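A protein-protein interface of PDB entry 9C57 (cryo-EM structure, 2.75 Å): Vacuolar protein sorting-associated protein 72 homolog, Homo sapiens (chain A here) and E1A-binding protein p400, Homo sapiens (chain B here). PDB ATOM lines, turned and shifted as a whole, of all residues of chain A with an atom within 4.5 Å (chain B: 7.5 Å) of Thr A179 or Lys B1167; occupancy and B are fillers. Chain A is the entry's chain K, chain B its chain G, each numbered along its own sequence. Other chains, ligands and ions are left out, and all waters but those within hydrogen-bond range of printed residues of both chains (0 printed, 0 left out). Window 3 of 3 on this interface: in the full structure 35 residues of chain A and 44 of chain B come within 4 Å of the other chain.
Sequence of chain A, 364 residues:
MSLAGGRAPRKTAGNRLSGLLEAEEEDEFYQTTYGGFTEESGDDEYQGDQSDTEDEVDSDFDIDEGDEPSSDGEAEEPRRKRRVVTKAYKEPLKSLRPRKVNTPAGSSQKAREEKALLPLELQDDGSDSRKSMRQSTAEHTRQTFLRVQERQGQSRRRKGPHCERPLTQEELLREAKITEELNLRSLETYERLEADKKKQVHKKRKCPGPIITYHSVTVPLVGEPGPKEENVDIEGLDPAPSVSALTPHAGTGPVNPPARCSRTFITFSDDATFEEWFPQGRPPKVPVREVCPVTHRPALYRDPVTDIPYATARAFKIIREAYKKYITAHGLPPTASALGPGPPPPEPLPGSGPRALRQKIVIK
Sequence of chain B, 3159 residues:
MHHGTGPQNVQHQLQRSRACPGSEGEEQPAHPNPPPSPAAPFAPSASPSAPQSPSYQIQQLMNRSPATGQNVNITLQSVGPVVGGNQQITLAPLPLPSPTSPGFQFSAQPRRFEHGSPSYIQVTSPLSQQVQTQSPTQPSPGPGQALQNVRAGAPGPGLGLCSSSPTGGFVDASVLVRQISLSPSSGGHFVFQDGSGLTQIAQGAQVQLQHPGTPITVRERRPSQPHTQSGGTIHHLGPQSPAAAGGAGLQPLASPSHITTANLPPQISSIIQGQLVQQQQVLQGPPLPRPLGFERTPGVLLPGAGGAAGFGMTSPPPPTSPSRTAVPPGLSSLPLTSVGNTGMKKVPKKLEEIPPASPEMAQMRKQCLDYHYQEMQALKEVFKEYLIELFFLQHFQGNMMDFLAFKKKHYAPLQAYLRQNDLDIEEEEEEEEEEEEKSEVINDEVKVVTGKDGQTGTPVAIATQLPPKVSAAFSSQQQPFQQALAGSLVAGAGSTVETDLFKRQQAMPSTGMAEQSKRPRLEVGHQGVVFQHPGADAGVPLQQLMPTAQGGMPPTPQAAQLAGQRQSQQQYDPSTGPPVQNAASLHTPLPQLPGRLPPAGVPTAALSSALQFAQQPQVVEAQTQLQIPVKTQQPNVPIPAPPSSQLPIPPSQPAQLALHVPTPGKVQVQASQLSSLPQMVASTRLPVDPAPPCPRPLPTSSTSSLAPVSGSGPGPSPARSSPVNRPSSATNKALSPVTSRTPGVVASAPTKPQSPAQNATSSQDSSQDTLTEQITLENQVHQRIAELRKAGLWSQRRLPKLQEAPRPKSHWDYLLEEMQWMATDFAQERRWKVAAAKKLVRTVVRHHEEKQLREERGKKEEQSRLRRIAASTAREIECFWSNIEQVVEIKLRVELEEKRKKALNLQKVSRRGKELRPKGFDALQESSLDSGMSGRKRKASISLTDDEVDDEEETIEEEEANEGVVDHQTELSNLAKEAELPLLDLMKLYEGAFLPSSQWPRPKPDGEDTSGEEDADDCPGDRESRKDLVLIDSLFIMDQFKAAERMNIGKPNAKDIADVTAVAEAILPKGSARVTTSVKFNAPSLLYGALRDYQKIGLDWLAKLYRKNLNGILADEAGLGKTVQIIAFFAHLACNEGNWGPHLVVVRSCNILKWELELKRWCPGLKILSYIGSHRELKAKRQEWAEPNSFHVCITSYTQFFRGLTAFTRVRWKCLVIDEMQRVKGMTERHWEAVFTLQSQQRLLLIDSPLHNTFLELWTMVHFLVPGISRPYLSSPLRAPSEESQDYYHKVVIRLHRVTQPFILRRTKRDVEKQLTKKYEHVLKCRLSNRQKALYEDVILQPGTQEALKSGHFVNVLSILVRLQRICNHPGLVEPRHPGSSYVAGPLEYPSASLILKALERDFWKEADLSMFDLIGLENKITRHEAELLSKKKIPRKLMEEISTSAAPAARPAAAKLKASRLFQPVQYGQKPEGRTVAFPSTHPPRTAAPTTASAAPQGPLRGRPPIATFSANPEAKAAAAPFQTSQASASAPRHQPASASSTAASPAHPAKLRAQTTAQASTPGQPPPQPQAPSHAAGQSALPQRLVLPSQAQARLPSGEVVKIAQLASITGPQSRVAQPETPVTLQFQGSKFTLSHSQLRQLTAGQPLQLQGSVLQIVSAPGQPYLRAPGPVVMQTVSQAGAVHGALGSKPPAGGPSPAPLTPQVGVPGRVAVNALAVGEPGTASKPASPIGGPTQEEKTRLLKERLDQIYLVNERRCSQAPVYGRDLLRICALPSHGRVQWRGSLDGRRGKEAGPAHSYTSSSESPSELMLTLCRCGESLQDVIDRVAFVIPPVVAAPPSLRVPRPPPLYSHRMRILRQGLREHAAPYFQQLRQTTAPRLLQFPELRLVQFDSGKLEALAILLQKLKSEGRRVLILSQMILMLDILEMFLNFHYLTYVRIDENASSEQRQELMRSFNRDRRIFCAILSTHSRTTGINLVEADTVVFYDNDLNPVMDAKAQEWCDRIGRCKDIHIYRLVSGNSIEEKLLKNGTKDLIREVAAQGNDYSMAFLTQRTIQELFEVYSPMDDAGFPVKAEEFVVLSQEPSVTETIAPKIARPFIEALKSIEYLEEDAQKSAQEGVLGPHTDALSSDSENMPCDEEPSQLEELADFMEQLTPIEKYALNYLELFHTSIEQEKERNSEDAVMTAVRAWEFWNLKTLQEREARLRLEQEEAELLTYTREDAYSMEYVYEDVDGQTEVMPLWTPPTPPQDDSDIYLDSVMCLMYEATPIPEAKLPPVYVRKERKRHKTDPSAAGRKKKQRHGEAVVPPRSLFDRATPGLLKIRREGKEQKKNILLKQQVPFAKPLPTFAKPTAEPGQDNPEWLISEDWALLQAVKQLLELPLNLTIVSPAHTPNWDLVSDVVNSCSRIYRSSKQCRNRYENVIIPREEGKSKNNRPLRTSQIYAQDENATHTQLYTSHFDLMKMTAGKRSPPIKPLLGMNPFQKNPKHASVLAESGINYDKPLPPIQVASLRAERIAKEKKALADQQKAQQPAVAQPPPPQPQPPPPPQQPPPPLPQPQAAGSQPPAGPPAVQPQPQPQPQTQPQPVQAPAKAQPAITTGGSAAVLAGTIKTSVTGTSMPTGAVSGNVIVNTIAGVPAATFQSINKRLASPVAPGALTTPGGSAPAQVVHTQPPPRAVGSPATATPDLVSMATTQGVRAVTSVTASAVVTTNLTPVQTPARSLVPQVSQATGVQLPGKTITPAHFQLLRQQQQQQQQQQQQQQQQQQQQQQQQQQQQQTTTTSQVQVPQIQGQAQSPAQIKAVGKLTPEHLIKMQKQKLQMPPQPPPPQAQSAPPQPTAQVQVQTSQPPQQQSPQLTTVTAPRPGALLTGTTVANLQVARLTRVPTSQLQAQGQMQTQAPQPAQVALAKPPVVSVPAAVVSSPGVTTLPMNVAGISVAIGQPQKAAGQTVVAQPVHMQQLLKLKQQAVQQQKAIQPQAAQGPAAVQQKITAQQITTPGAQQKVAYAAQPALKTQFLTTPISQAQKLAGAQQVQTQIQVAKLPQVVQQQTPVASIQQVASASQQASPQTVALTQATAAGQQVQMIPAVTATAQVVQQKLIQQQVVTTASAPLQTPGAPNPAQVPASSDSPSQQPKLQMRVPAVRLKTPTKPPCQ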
ATOM      1  N   GLU A 175     -25.876  20.550 -13.144  1.00  0.00           N
ATOM      2  CA  GLU A 175     -25.077  21.707 -12.747  1.00  0.00           C
ATOM      3  C   GLU A 175     -25.492  22.911 -13.571  1.00  0.00           C
ATOM      4  O   GLU A 175     -25.187  24.039 -13.189  1.00  0.00           O
ATOM      5  CB  GLU A 175     -23.559  21.542 -12.912  1.00  0.00           C
ATOM      6  CG  GLU A 175     -22.954  21.642 -14.300  1.00  0.00           C
ATOM      7  CD  GLU A 175     -23.669  20.889 -15.375  1.00  0.00           C
ATOM      8  OE1 GLU A 175     -24.674  20.244 -15.063  1.00  0.00           O
ATOM      9  OE2 GLU A 175     -23.194  20.910 -16.531  1.00  0.00           O
ATOM     10  N   ALA A 176     -26.197  22.691 -14.688  1.00  0.00           N
ATOM     11  CA  ALA A 176     -26.712  23.796 -15.483  1.00  0.00           C
ATOM     12  C   ALA A 176     -27.866  24.488 -14.777  1.00  0.00           C
ATOM     13  O   ALA A 176     -27.982  25.712 -14.835  1.00  0.00           O
ATOM     14  CB  ALA A 176     -27.154  23.291 -16.857  1.00  0.00           C
ATOM     15  N   LYS A 177     -28.735  23.730 -14.105  1.00  0.00           N
ATOM     16  CA  LYS A 177     -29.759  24.381 -13.294  1.00  0.00           C
ATOM     17  C   LYS A 177     -29.129  25.094 -12.103  1.00  0.00           C
ATOM     18  O   LYS A 177     -29.564  26.192 -11.722  1.00  0.00           O
ATOM     19  CB  LYS A 177     -30.796  23.361 -12.828  1.00  0.00           C
ATOM     20  CG  LYS A 177     -31.764  22.815 -13.899  1.00  0.00           C
ATOM     21  CD  LYS A 177     -32.170  23.800 -15.012  1.00  0.00           C
ATOM     22  CE  LYS A 177     -31.154  23.911 -16.151  1.00  0.00           C
ATOM     23  NZ  LYS A 177     -31.568  24.922 -17.162  1.00  0.00           N
ATOM     24  N   ILE A 178     -28.095  24.496 -11.509  1.00  0.00           N
ATOM     25  CA  ILE A 178     -27.383  25.196 -10.439  1.00  0.00           C
ATOM     26  C   ILE A 178     -26.782  26.497 -10.966  1.00  0.00           C
ATOM     27  O   ILE A 178     -26.855  27.551 -10.316  1.00  0.00           O
ATOM     28  CB  ILE A 178     -26.311  24.280  -9.818  1.00  0.00           C
ATOM     29  CG1 ILE A 178     -26.970  23.086  -9.118  1.00  0.00           C
ATOM     30  CG2 ILE A 178     -25.434  25.059  -8.847  1.00  0.00           C
ATOM     31  CD1 ILE A 178     -27.784  23.448  -7.881  1.00  0.00           C
ATOM     32  N   THR A 179     -26.185  26.442 -12.156  1.00  0.00           N
ATOM     33  CA  THR A 179     -25.628  27.630 -12.789  1.00  0.00           C
ATOM     34  C   THR A 179     -26.715  28.652 -13.078  1.00  0.00           C
ATOM     35  O   THR A 179     -26.492  29.861 -12.959  1.00  0.00           O
ATOM     36  CB  THR A 179     -24.923  27.234 -14.083  1.00  0.00           C
ATOM     37  OG1 THR A 179     -24.002  26.169 -13.819  1.00  0.00           O
ATOM     38  CG2 THR A 179     -24.178  28.413 -14.671  1.00  0.00           C
ATOM     39  N   GLU A 180     -27.887  28.184 -13.494  1.00  0.00           N
ATOM     40  CA  GLU A 180     -29.027  29.068 -13.677  1.00  0.00           C
ATOM     41  C   GLU A 180     -29.305  29.847 -12.406  1.00  0.00           C
ATOM     42  O   GLU A 180     -29.362  31.081 -12.415  1.00  0.00           O
ATOM     43  CB  GLU A 180     -30.254  28.237 -14.067  1.00  0.00           C
ATOM     44  CG  GLU A 180     -31.190  28.860 -15.079  1.00  0.00           C
ATOM     45  CD  GLU A 180     -30.486  29.447 -16.284  1.00  0.00           C
ATOM     46  OE1 GLU A 180     -29.259  29.273 -16.438  1.00  0.00           O
ATOM     47  OE2 GLU A 180     -31.172  30.116 -17.072  1.00  0.00           O
ATOM     48  N   GLU A 181     -29.447  29.140 -11.289  1.00  0.00           N
ATOM     49  CA  GLU A 181     -29.751  29.829 -10.042  1.00  0.00           C
ATOM     50  C   GLU A 181     -28.655  30.834  -9.724  1.00  0.00           C
ATOM     51  O   GLU A 181     -28.936  31.992  -9.391  1.00  0.00           O
ATOM     52  CB  GLU A 181     -29.945  28.805  -8.915  1.00  0.00           C
ATOM     53  CG  GLU A 181     -30.655  29.311  -7.635  1.00  0.00           C
ATOM     54  CD  GLU A 181     -30.023  30.519  -6.945  1.00  0.00           C
ATOM     55  OE1 GLU A 181     -28.870  30.882  -7.237  1.00  0.00           O
ATOM     56  OE2 GLU A 181     -30.720  31.157  -6.132  1.00  0.00           O
ATOM     57  N   LEU A 182     -27.397  30.423  -9.855  1.00  0.00           N
ATOM     58  CA  LEU A 182     -26.300  31.296  -9.446  1.00  0.00           C
ATOM     59  C   LEU A 182     -26.243  32.550 -10.313  1.00  0.00           C
ATOM     60  O   LEU A 182     -26.143  33.670  -9.799  1.00  0.00           O
ATOM     61  CB  LEU A 182     -24.980  30.527  -9.509  1.00  0.00           C
ATOM     62  CG  LEU A 182     -23.689  31.263  -9.128  1.00  0.00           C
ATOM     63  CD1 LEU A 182     -23.067  31.959 -10.335  1.00  0.00           C
ATOM     64  CD2 LEU A 182     -23.905  32.239  -7.970  1.00  0.00           C
ATOM     65  N   ASN A 183     -26.306  32.382 -11.635  1.00  0.00           N
ATOM     66  CA  ASN A 183     -26.137  33.516 -12.539  1.00  0.00           C
ATOM     67  C   ASN A 183     -27.328  34.464 -12.481  1.00  0.00           C
ATOM     68  O   ASN A 183     -27.154  35.684 -12.388  1.00  0.00           O
ATOM     69  CB  ASN A 183     -25.920  33.019 -13.968  1.00  0.00           C
ATOM     70  CG  ASN A 183     -24.831  31.977 -14.061  1.00  0.00           C
ATOM     71  OD1 ASN A 183     -24.382  31.436 -13.052  1.00  0.00           O
ATOM     72  ND2 ASN A 183     -24.393  31.693 -15.282  1.00  0.00           N
ATOM     73  N   LEU B1086     -29.353  26.591 -22.779  1.00  0.00           N
ATOM     74  CA  LEU B1086     -28.607  27.708 -22.211  1.00  0.00           C
ATOM     75  C   LEU B1086     -29.152  29.057 -22.666  1.00  0.00           C
ATOM     76  O   LEU B1086     -29.252  29.984 -21.854  1.00  0.00           O
ATOM     77  CB  LEU B1086     -27.131  27.595 -22.593  1.00  0.00           C
ATOM     78  CG  LEU B1086     -26.376  26.418 -21.980  1.00  0.00           C
ATOM     79  CD1 LEU B1086     -25.025  26.248 -22.655  1.00  0.00           C
ATOM     80  CD2 LEU B1086     -26.210  26.606 -20.487  1.00  0.00           C
ATOM     81  N   PHE B1130     -21.927  29.828 -28.766  1.00  0.00           N
ATOM     82  CA  PHE B1130     -21.475  29.058 -27.614  1.00  0.00           C
ATOM     83  C   PHE B1130     -22.582  28.143 -27.110  1.00  0.00           C
ATOM     84  O   PHE B1130     -22.341  26.972 -26.794  1.00  0.00           O
ATOM     85  CB  PHE B1130     -21.021  30.004 -26.503  1.00  0.00           C
ATOM     86  CG  PHE B1130     -19.718  29.616 -25.871  1.00  0.00           C
ATOM     87  CD1 PHE B1130     -19.686  28.722 -24.815  1.00  0.00           C
ATOM     88  CD2 PHE B1130     -18.527  30.153 -26.324  1.00  0.00           C
ATOM     89  CE1 PHE B1130     -18.490  28.364 -24.228  1.00  0.00           C
ATOM     90  CE2 PHE B1130     -17.325  29.801 -25.740  1.00  0.00           C
ATOM     91  CZ  PHE B1130     -17.307  28.905 -24.690  1.00  0.00           C
ATOM     92  N   LEU B1159     -22.830  37.259 -21.313  1.00  0.00           N
ATOM     93  CA  LEU B1159     -22.806  35.808 -21.153  1.00  0.00           C
ATOM     94  C   LEU B1159     -23.859  35.354 -20.148  1.00  0.00           C
ATOM     95  O   LEU B1159     -24.683  34.482 -20.444  1.00  0.00           O
ATOM     96  CB  LEU B1159     -21.415  35.347 -20.712  1.00  0.00           C
ATOM     97  CG  LEU B1159     -20.369  34.932 -21.756  1.00  0.00           C
ATOM     98  CD1 LEU B1159     -20.919  33.908 -22.744  1.00  0.00           C
ATOM     99  CD2 LEU B1159     -19.815  36.137 -22.499  1.00  0.00           C
ATOM    100  N   LYS B1160     -23.850  35.946 -18.953  1.00  0.00           N
ATOM    101  CA  LYS B1160     -24.831  35.584 -17.936  1.00  0.00           C
ATOM    102  C   LYS B1160     -26.245  35.914 -18.387  1.00  0.00           C
ATOM    103  O   LYS B1160     -27.201  35.244 -17.983  1.00  0.00           O
ATOM    104  CB  LYS B1160     -24.525  36.310 -16.626  1.00  0.00           C
ATOM    105  CG  LYS B1160     -23.271  35.830 -15.923  1.00  0.00           C
ATOM    106  CD  LYS B1160     -22.887  36.766 -14.789  1.00  0.00           C
ATOM    107  CE  LYS B1160     -21.765  36.190 -13.942  1.00  0.00           C
ATOM    108  NZ  LYS B1160     -21.287  37.158 -12.917  1.00  0.00           N
ATOM    109  N   CYS B1163     -27.069  33.571 -21.836  1.00  0.00           N
ATOM    110  CA  CYS B1163     -26.758  32.173 -21.543  1.00  0.00           C
ATOM    111  C   CYS B1163     -26.362  32.042 -20.081  1.00  0.00           C
ATOM    112  O   CYS B1163     -25.196  31.789 -19.752  1.00  0.00           O
ATOM    113  CB  CYS B1163     -25.650  31.662 -22.463  1.00  0.00           C
ATOM    114  SG  CYS B1163     -26.195  31.425 -24.161  1.00  0.00           S
ATOM    115  N   PRO B1164     -27.320  32.204 -19.167  1.00  0.00           N
ATOM    116  CA  PRO B1164     -26.996  32.127 -17.734  1.00  0.00           C
ATOM    117  C   PRO B1164     -26.563  30.750 -17.266  1.00  0.00           C
ATOM    118  O   PRO B1164     -26.135  30.624 -16.113  1.00  0.00           O
ATOM    119  CB  PRO B1164     -28.305  32.552 -17.053  1.00  0.00           C
ATOM    120  CG  PRO B1164     -29.360  32.357 -18.091  1.00  0.00           C
ATOM    121  CD  PRO B1164     -28.711  32.621 -19.400  1.00  0.00           C
ATOM    122  N   GLY B1165     -26.669  29.718 -18.097  1.00  0.00           N
ATOM    123  CA  GLY B1165     -26.365  28.372 -17.657  1.00  0.00           C
ATOM    124  C   GLY B1165     -24.914  27.960 -17.732  1.00  0.00           C
ATOM    125  O   GLY B1165     -24.594  26.808 -17.426  1.00  0.00           O
ATOM    126  N   LEU B1166     -24.020  28.861 -18.124  1.00  0.00           N
ATOM    127  CA  LEU B1166     -22.605  28.548 -18.281  1.00  0.00           C
ATOM    128  C   LEU B1166     -21.828  29.035 -17.067  1.00  0.00           C
ATOM    129  O   LEU B1166     -22.039  30.160 -16.601  1.00  0.00           O
ATOM    130  CB  LEU B1166     -22.046  29.200 -19.547  1.00  0.00           C
ATOM    131  CG  LEU B1166     -22.626  28.728 -20.881  1.00  0.00           C
ATOM    132  CD1 LEU B1166     -22.393  29.777 -21.957  1.00  0.00           C
ATOM    133  CD2 LEU B1166     -22.017  27.397 -21.290  1.00  0.00           C
ATOM    134  N   LYS B1167     -20.934  28.192 -16.556  1.00  0.00           N
ATOM    135  CA  LYS B1167     -20.016  28.641 -15.521  1.00  0.00           C
ATOM    136  C   LYS B1167     -19.068  29.681 -16.098  1.00  0.00           C
ATOM    137  O   LYS B1167     -18.574  29.541 -17.220  1.00  0.00           O
ATOM    138  CB  LYS B1167     -19.216  27.466 -14.951  1.00  0.00           C
ATOM    139  CG  LYS B1167     -20.040  26.306 -14.400  1.00  0.00           C
ATOM    140  CD  LYS B1167     -21.277  26.747 -13.630  1.00  0.00           C
ATOM    141  CE  LYS B1167     -20.966  27.715 -12.493  1.00  0.00           C
ATOM    142  NZ  LYS B1167     -22.180  27.994 -11.675  1.00  0.00           N
ATOM    143  N   ILE B1168     -18.812  30.730 -15.323  1.00  0.00           N
ATOM    144  CA  ILE B1168     -17.993  31.851 -15.760  1.00  0.00           C
ATOM    145  C   ILE B1168     -16.791  31.967 -14.837  1.00  0.00           C
ATOM    146  O   ILE B1168     -16.930  31.928 -13.610  1.00  0.00           O
ATOM    147  CB  ILE B1168     -18.794  33.170 -15.778  1.00  0.00           C
ATOM    148  CG1 ILE B1168     -20.100  32.997 -16.560  1.00  0.00           C
ATOM    149  CG2 ILE B1168     -17.957  34.289 -16.379  1.00  0.00           C
ATOM    150  CD1 ILE B1168     -19.913  32.578 -18.007  1.00  0.00           C
ATOM    151  N   LEU B1169     -15.610  32.102 -15.433  1.00  0.00           N
ATOM    152  CA  LEU B1169     -14.374  32.325 -14.700  1.00  0.00           C
ATOM    153  C   LEU B1169     -13.848  33.706 -15.058  1.00  0.00           C
ATOM    154  O   LEU B1169     -13.697  34.028 -16.241  1.00  0.00           O
ATOM    155  CB  LEU B1169     -13.340  31.239 -15.025  1.00  0.00           C
ATOM    156  CG  LEU B1169     -11.875  31.458 -14.632  1.00  0.00           C
ATOM    157  CD1 LEU B1169     -11.175  30.116 -14.560  1.00  0.00           C
ATOM    158  CD2 LEU B1169     -11.122  32.357 -15.607  1.00  0.00           C
ATOM    159  N   ASN B1189     -13.724  20.361 -14.395  1.00  0.00           N
ATOM    160  CA  ASN B1189     -15.106  20.808 -14.219  1.00  0.00           C
ATOM    161  C   ASN B1189     -15.188  22.048 -13.332  1.00  0.00           C
ATOM    162  O   ASN B1189     -16.135  22.219 -12.562  1.00  0.00           O
ATOM    163  CB  ASN B1189     -15.975  19.685 -13.649  1.00  0.00           C
ATOM    164  CG  ASN B1189     -15.907  18.419 -14.480  1.00  0.00           C
ATOM    165  OD1 ASN B1189     -15.604  18.462 -15.674  1.00  0.00           O
ATOM    166  ND2 ASN B1189     -16.191  17.282 -13.855  1.00  0.00           N
ATOM    167  N   SER B1190     -14.189  22.922 -13.440  1.00  0.00           N
ATOM    168  CA  SER B1190     -14.144  24.129 -12.625  1.00  0.00           C
ATOM    169  C   SER B1190     -14.908  25.289 -13.246  1.00  0.00           C
ATOM    170  O   SER B1190     -15.467  26.114 -12.514  1.00  0.00           O
ATOM    171  CB  SER B1190     -12.689  24.544 -12.393  1.00  0.00           C
ATOM    172  OG  SER B1190     -11.945  24.488 -13.598  1.00  0.00           O
ATOM    173  N   PHE B1191     -14.949  25.370 -14.572  1.00  0.00           N
ATOM    174  CA  PHE B1191     -15.604  26.478 -15.254  1.00  0.00           C
ATOM    175  C   PHE B1191     -15.959  26.036 -16.665  1.00  0.00           C
ATOM    176  O   PHE B1191     -15.559  24.963 -17.122  1.00  0.00           O
ATOM    177  CB  PHE B1191     -14.706  27.717 -15.291  1.00  0.00           C
ATOM    178  CG  PHE B1191     -13.616  27.635 -16.316  1.00  0.00           C
ATOM    179  CD1 PHE B1191     -12.444  26.954 -16.042  1.00  0.00           C
ATOM    180  CD2 PHE B1191     -13.768  28.227 -17.559  1.00  0.00           C
ATOM    181  CE1 PHE B1191     -11.439  26.870 -16.983  1.00  0.00           C
ATOM    182  CE2 PHE B1191     -12.766  28.145 -18.507  1.00  0.00           C
ATOM    183  CZ  PHE B1191     -11.599  27.465 -18.216  1.00  0.00           C
ATOM    184  N   HIS B1192     -16.723  26.884 -17.350  1.00  0.00           N
ATOM    185  CA  HIS B1192     -17.082  26.672 -18.746  1.00  0.00           C
ATOM    186  C   HIS B1192     -16.487  27.726 -19.667  1.00  0.00           C
ATOM    187  O   HIS B1192     -15.912  27.388 -20.706  1.00  0.00           O
ATOM    188  CB  HIS B1192     -18.609  26.654 -18.897  1.00  0.00           C
ATOM    189  CG  HIS B1192     -19.258  25.435 -18.321  1.00  0.00           C
ATOM    190  ND1 HIS B1192     -20.387  24.865 -18.869  1.00  0.00           N
ATOM    191  CD2 HIS B1192     -18.934  24.674 -17.250  1.00  0.00           C
ATOM    192  CE1 HIS B1192     -20.732  23.807 -18.158  1.00  0.00           C
ATOM    193  NE2 HIS B1192     -19.867  23.669 -17.170  1.00  0.00           N
ATOM    194  N   VAL B1193     -16.608  29.002 -19.308  1.00  0.00           N
ATOM    195  CA  VAL B1193     -16.094  30.108 -20.105  1.00  0.00           C
ATOM    196  C   VAL B1193     -15.114  30.897 -19.253  1.00  0.00           C
ATOM    197  O   VAL B1193     -15.438  31.285 -18.124  1.00  0.00           O
ATOM    198  CB  VAL B1193     -17.226  31.019 -20.611  1.00  0.00           C
ATOM    199  CG1 VAL B1193     -16.673  32.090 -21.539  1.00  0.00           C
ATOM    200  CG2 VAL B1193     -18.298  30.196 -21.304  1.00  0.00           C
ATOM    201  N   CYS B1194     -13.924  31.137 -19.791  1.00  0.00           N
ATOM    202  CA  CYS B1194     -12.911  31.950 -19.136  1.00  0.00           C
ATOM    203  C   CYS B1194     -12.811  33.289 -19.850  1.00  0.00           C
ATOM    204  O   CYS B1194     -12.677  33.334 -21.078  1.00  0.00           O
ATOM    205  CB  CYS B1194     -11.552  31.251 -19.140  1.00  0.00           C
ATOM    206  SG  CYS B1194     -10.149  32.373 -18.932  1.00  0.00           S
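Among the printed residues, merely in contact across the chains: Thr A179 with Gly B1165 and Thr A179 with Leu B1166.
Lys B1167 touches just one residue of chain A: Thr A179. Of the printed residues of chain A, Leu B1166 touches Thr A179 and Asn A183. Of the printed residues of chain B, Asn A183 touches Pro B1164 and Leu B1166. Of the printed residues of chain A, Pro B1164 touches Thr A179, Glu A180 and Asn A183. Printed residues of chain B within 4 Å of Glu A180: Pro B1164 and Gly B1165.
ND2 of Asn A183 is in hydrogen-bond range of O of Leu B1166, at 3.1 Å. O of Thr A179 lies close to O of Pro B1164 (3.3 Å). The backbone carbonyl oxygen of Pro B1164 lies close to the side-chain amide nitrogen of Asn A183 (2.2 Å). The backbone carbonyl oxygen (O) of Pro B1164 sits close to the side-chain carboxylate (OE1) of Glu A180 (3.4 Å). The side-chain carboxylate (OE1) of Glu A180 sits at hydrogen-bond distance from the backbone NH (N) of Gly B1165. The side-chain hydroxyl (OG1) of Thr A179 lies close to the side-chain amino group (NZ) of Lys B1167, 3.4 Å away.
Of the 17 printed residues of chain B, 4 touch a printed residue of chain A. Printed residues of chain A that touch a printed residue of chain B: Thr A179, Glu A180 and Asn A183. Among the printed residues, 8 pairs touch across the chains. Among the printed residues, no Asp or Glu carboxylate lies within 4 Å of a Lys or Arg side-chain nitrogen of the other chain.
The backbone carbonyl oxygen of Lys B1167 is in hydrogen-bond range of the backbone NH of His B1192 (3.2 Å). The backbone carbonyl oxygen of Lys B1167 lies within hydrogen-bond range of the backbone NH of Val B1193 (2.9 Å). The backbone carbonyl oxygen (O) of Thr A179 sits close to the side-chain amide oxygen (OD1) of Asn A183, at 2.6 Å. O of Glu A175 lies within hydrogen-bond range of OG1 of Thr A179 (2.5 Å).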
